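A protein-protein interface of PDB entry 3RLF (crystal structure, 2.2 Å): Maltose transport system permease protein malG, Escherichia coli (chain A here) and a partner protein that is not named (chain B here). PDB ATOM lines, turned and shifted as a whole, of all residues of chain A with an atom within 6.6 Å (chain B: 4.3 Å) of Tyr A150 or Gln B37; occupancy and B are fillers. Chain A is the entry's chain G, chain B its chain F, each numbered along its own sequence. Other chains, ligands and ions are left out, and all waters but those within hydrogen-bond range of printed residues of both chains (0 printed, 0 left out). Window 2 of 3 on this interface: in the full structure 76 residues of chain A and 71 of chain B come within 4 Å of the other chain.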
ATOM      1  N   ASP A 145      -8.372  -7.648 -17.432  1.00  0.00           N
ATOM      2  CA  ASP A 145      -8.018  -8.401 -16.230  1.00  0.00           C
ATOM      3  C   ASP A 145      -6.646  -7.947 -15.743  1.00  0.00           C
ATOM      4  O   ASP A 145      -6.447  -7.726 -14.550  1.00  0.00           O
ATOM      5  CB  ASP A 145      -8.024  -9.906 -16.506  1.00  0.00           C
ATOM      6  CG  ASP A 145      -8.120 -10.740 -15.237  1.00  0.00           C
ATOM      7  OD1 ASP A 145      -8.647 -10.244 -14.215  1.00  0.00           O
ATOM      8  OD2 ASP A 145      -7.674 -11.908 -15.268  1.00  0.00           O
ATOM      9  N   ARG A 146      -5.719  -7.790 -16.687  1.00  0.00           N
ATOM     10  CA  ARG A 146      -4.380  -7.276 -16.412  1.00  0.00           C
ATOM     11  C   ARG A 146      -4.397  -5.804 -15.994  1.00  0.00           C
ATOM     12  O   ARG A 146      -3.700  -5.413 -15.059  1.00  0.00           O
ATOM     13  CB  ARG A 146      -3.469  -7.471 -17.634  1.00  0.00           C
ATOM     14  CG  ARG A 146      -2.564  -8.706 -17.581  1.00  0.00           C
ATOM     15  CD  ARG A 146      -3.330 -10.023 -17.691  1.00  0.00           C
ATOM     16  NE  ARG A 146      -2.434 -11.181 -17.659  1.00  0.00           N
ATOM     17  CZ  ARG A 146      -2.837 -12.445 -17.549  1.00  0.00           C
ATOM     18  NH1 ARG A 146      -4.130 -12.735 -17.455  1.00  0.00           N
ATOM     19  NH2 ARG A 146      -1.943 -13.425 -17.527  1.00  0.00           N
ATOM     20  N   LEU A 147      -5.200  -5.001 -16.688  1.00  0.00           N
ATOM     21  CA  LEU A 147      -5.296  -3.563 -16.431  1.00  0.00           C
ATOM     22  C   LEU A 147      -5.851  -3.253 -15.036  1.00  0.00           C
ATOM     23  O   LEU A 147      -5.417  -2.295 -14.389  1.00  0.00           O
ATOM     24  CB  LEU A 147      -6.159  -2.899 -17.515  1.00  0.00           C
ATOM     25  CG  LEU A 147      -6.193  -1.376 -17.682  1.00  0.00           C
ATOM     26  CD1 LEU A 147      -4.911  -0.848 -18.311  1.00  0.00           C
ATOM     27  CD2 LEU A 147      -7.395  -0.980 -18.526  1.00  0.00           C
ATOM     28  N   GLY A 148      -6.791  -4.081 -14.580  1.00  0.00           N
ATOM     29  CA  GLY A 148      -7.503  -3.874 -13.317  1.00  0.00           C
ATOM     30  C   GLY A 148      -6.680  -3.942 -12.043  1.00  0.00           C
ATOM     31  O   GLY A 148      -7.022  -3.296 -11.049  1.00  0.00           O
ATOM     32  N   GLU A 149      -5.602  -4.723 -12.062  1.00  0.00           N
ATOM     33  CA  GLU A 149      -4.725  -4.850 -10.894  1.00  0.00           C
ATOM     34  C   GLU A 149      -3.825  -3.624 -10.684  1.00  0.00           C
ATOM     35  O   GLU A 149      -3.217  -3.470  -9.622  1.00  0.00           O
ATOM     36  CB  GLU A 149      -3.903  -6.149 -10.947  1.00  0.00           C
ATOM     37  CG  GLU A 149      -2.953  -6.269 -12.133  1.00  0.00           C
ATOM     38  CD  GLU A 149      -2.216  -7.603 -12.188  1.00  0.00           C
ATOM     39  OE1 GLU A 149      -1.628  -8.020 -11.162  1.00  0.00           O
ATOM     40  OE2 GLU A 149      -2.212  -8.228 -13.271  1.00  0.00           O
ATOM     41  N   TYR A 150      -3.753  -2.754 -11.692  1.00  0.00           N
ATOM     42  CA  TYR A 150      -2.975  -1.517 -11.597  1.00  0.00           C
ATOM     43  C   TYR A 150      -3.871  -0.280 -11.510  1.00  0.00           C
ATOM     44  O   TYR A 150      -3.719   0.534 -10.598  1.00  0.00           O
ATOM     45  CB  TYR A 150      -1.987  -1.400 -12.765  1.00  0.00           C
ATOM     46  CG  TYR A 150      -1.119  -2.627 -12.953  1.00  0.00           C
ATOM     47  CD1 TYR A 150      -1.325  -3.487 -14.031  1.00  0.00           C
ATOM     48  CD2 TYR A 150      -0.103  -2.935 -12.050  1.00  0.00           C
ATOM     49  CE1 TYR A 150      -0.536  -4.619 -14.211  1.00  0.00           C
ATOM     50  CE2 TYR A 150       0.691  -4.066 -12.219  1.00  0.00           C
ATOM     51  CZ  TYR A 150       0.466  -4.905 -13.301  1.00  0.00           C
ATOM     52  OH  TYR A 150       1.252  -6.023 -13.473  1.00  0.00           O
ATOM     53  N   ILE A 151      -4.798  -0.145 -12.457  1.00  0.00           N
ATOM     54  CA  ILE A 151      -5.786   0.937 -12.431  1.00  0.00           C
ATOM     55  C   ILE A 151      -7.188   0.343 -12.238  1.00  0.00           C
ATOM     56  O   ILE A 151      -7.759  -0.232 -13.170  1.00  0.00           O
ATOM     57  CB  ILE A 151      -5.729   1.841 -13.699  1.00  0.00           C
ATOM     58  CG1 ILE A 151      -4.329   2.432 -13.900  1.00  0.00           C
ATOM     59  CG2 ILE A 151      -6.742   2.974 -13.597  1.00  0.00           C
ATOM     60  CD1 ILE A 151      -3.462   1.666 -14.885  1.00  0.00           C
ATOM     61  N   PRO A 152      -7.741   0.480 -11.019  1.00  0.00           N
ATOM     62  CA  PRO A 152      -8.995  -0.178 -10.645  1.00  0.00           C
ATOM     63  C   PRO A 152     -10.238   0.340 -11.376  1.00  0.00           C
ATOM     64  O   PRO A 152     -11.121  -0.456 -11.709  1.00  0.00           O
ATOM     65  CB  PRO A 152      -9.110   0.109  -9.137  1.00  0.00           C
ATOM     66  CG  PRO A 152      -7.747   0.553  -8.710  1.00  0.00           C
ATOM     67  CD  PRO A 152      -7.177   1.248  -9.895  1.00  0.00           C
ATOM     68  N   LEU B  33       7.269  -2.397 -11.415  1.00  0.00           N
ATOM     69  CA  LEU B  33       6.259  -3.131 -10.653  1.00  0.00           C
ATOM     70  C   LEU B  33       5.628  -4.244 -11.495  1.00  0.00           C
ATOM     71  O   LEU B  33       5.291  -5.309 -10.974  1.00  0.00           O
ATOM     72  CB  LEU B  33       5.186  -2.165 -10.130  1.00  0.00           C
ATOM     73  CG  LEU B  33       4.200  -2.529  -9.005  1.00  0.00           C
ATOM     74  CD1 LEU B  33       2.954  -3.232  -9.539  1.00  0.00           C
ATOM     75  CD2 LEU B  33       4.839  -3.340  -7.872  1.00  0.00           C
ATOM     76  N   MET B  34       5.477  -3.986 -12.793  1.00  0.00           N
ATOM     77  CA  MET B  34       4.963  -4.979 -13.739  1.00  0.00           C
ATOM     78  C   MET B  34       6.011  -6.040 -14.065  1.00  0.00           C
ATOM     79  O   MET B  34       5.667  -7.175 -14.401  1.00  0.00           O
ATOM     80  CB  MET B  34       4.494  -4.306 -15.030  1.00  0.00           C
ATOM     81  CG  MET B  34       3.232  -3.479 -14.885  1.00  0.00           C
ATOM     82  SD  MET B  34       3.029  -2.316 -16.246  1.00  0.00           S
ATOM     83  CE  MET B  34       1.739  -1.256 -15.598  1.00  0.00           C
ATOM     84  N   ALA B  36       7.940  -7.403 -11.972  1.00  0.00           N
ATOM     85  CA  ALA B  36       7.792  -8.399 -10.912  1.00  0.00           C
ATOM     86  C   ALA B  36       6.650  -9.373 -11.225  1.00  0.00           C
ATOM     87  O   ALA B  36       6.049  -9.303 -12.298  1.00  0.00           O
ATOM     88  CB  ALA B  36       7.572  -7.715  -9.567  1.00  0.00           C
ATOM     89  N   GLN B  37       6.355 -10.263 -10.275  1.00  0.00           N
ATOM     90  CA  GLN B  37       5.389 -11.377 -10.428  1.00  0.00           C
ATOM     91  C   GLN B  37       5.474 -12.178 -11.744  1.00  0.00           C
ATOM     92  O   GLN B  37       5.662 -13.399 -11.714  1.00  0.00           O
ATOM     93  CB  GLN B  37       3.937 -10.967 -10.083  1.00  0.00           C
ATOM     94  CG  GLN B  37       3.280  -9.902 -10.967  1.00  0.00           C
ATOM     95  CD  GLN B  37       3.500  -8.482 -10.467  1.00  0.00           C
ATOM     96  OE1 GLN B  37       4.171  -8.256  -9.459  1.00  0.00           O
ATOM     97  NE2 GLN B  37       2.930  -7.515 -11.177  1.00  0.00           N
ATOM     98  N   GLY B  38       5.339 -11.489 -12.879  1.00  0.00           N
ATOM     99  CA  GLY B  38       5.466 -12.108 -14.196  1.00  0.00           C
ATOM    100  C   GLY B  38       4.518 -11.526 -15.226  1.00  0.00           C
ATOM    101  O   GLY B  38       3.644 -12.227 -15.741  1.00  0.00           O
ATOM    102  N   GLU B  39       4.692 -10.240 -15.524  1.00  0.00           N
ATOM    103  CA  GLU B  39       3.857  -9.539 -16.502  1.00  0.00           C
ATOM    104  C   GLU B  39       4.726  -8.848 -17.551  1.00  0.00           C
ATOM    105  O   GLU B  39       4.763  -7.617 -17.633  1.00  0.00           O
ATOM    106  CB  GLU B  39       2.938  -8.529 -15.802  1.00  0.00           C
ATOM    107  CG  GLU B  39       1.777  -9.148 -15.020  1.00  0.00           C
ATOM    108  CD  GLU B  39       0.622  -9.597 -15.907  1.00  0.00           C
ATOM    109  OE1 GLU B  39       0.563  -9.184 -17.086  1.00  0.00           O
ATOM    110  OE2 GLU B  39      -0.235 -10.362 -15.419  1.00  0.00           O
ATOM    111  N   PHE B  42       2.935  -7.113 -20.768  1.00  0.00           N
ATOM    112  CA  PHE B  42       2.311  -5.872 -20.321  1.00  0.00           C
ATOM    113  C   PHE B  42       3.342  -4.793 -19.981  1.00  0.00           C
ATOM    114  O   PHE B  42       3.041  -3.603 -20.048  1.00  0.00           O
ATOM    115  CB  PHE B  42       1.396  -6.137 -19.122  1.00  0.00           C
ATOM    116  CG  PHE B  42       0.319  -5.106 -18.942  1.00  0.00           C
ATOM    117  CD1 PHE B  42       0.468  -4.081 -18.014  1.00  0.00           C
ATOM    118  CD2 PHE B  42      -0.848  -5.159 -19.700  1.00  0.00           C
ATOM    119  CE1 PHE B  42      -0.528  -3.121 -17.843  1.00  0.00           C
ATOM    120  CE2 PHE B  42      -1.850  -4.204 -19.538  1.00  0.00           C
ATOM    121  CZ  PHE B  42      -1.690  -3.183 -18.607  1.00  0.00           C
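The side-chain hydroxyl (OH) of Tyr A150 is in hydrogen-bond range of the side-chain amide nitrogen (NE2) of Gln B37 (3.2 Å).
The guanidinium group (NE) of Arg A146 is in salt-bridge range of the side-chain carboxylate (OE2) of Glu B39.
The backbone carbonyl oxygen (O) of Leu B33 is in hydrogen-bond range of the side-chain amide nitrogen (NE2) of Gln B37 (3.2 Å).
N of Glu B39 lies close to O of Met B34.
Among the printed residues, merely in contact across the chains: Leu A147 with Phe B42 (3.99 Å), Glu A149 with Glu B39 (3.6 Å), Tyr A150 with Leu B33 (3.6 Å), Tyr A150 with Met B34 (3.5 Å), Tyr A150 with Glu B39 (3.5 Å) and Tyr A150 with Phe B42 (3.9 Å).
Tyr A150 touches just these residues of chain B: Leu B33, Met B34, Gln B37, Glu B39 and Phe B42.
Of chain A, only Tyr A150 comes within 4 Å of Gln B37.
Of the printed residues of chain B, Arg A146 touches Glu B39.
Of the printed residues of chain B, Leu A147 touches Phe B42.
Printed residues of chain A within 4 Å of Met B34: Tyr A150 (3.5 Å).
Printed residues of chain A within 4 Å of Glu B39: Arg A146, Glu A149 and Tyr A150.
Printed residues of chain B within 4 Å of Glu A149: Glu B39.
Pro A152 touches none of the printed residues of chain B.
Ile A151 touches none of the printed residues of chain B.
The nearest printed residue of chain A that does not touch Met B34 is Ile A151 (6.0 Å).
Of the 7 printed residues of chain B, 5 touch a printed residue of chain A.
Printed residues of chain B that touch a printed residue of chain A: Leu B33, Met B34, Gln B37, Glu B39 and Phe B42.
Hydrophobic or aromatic side chains of chain B within 4 Å of the printed part of chain A: Leu B33, Met B34 and Phe B42.
Of the 8 printed residues of chain A, 4 touch a printed residue of chain B.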
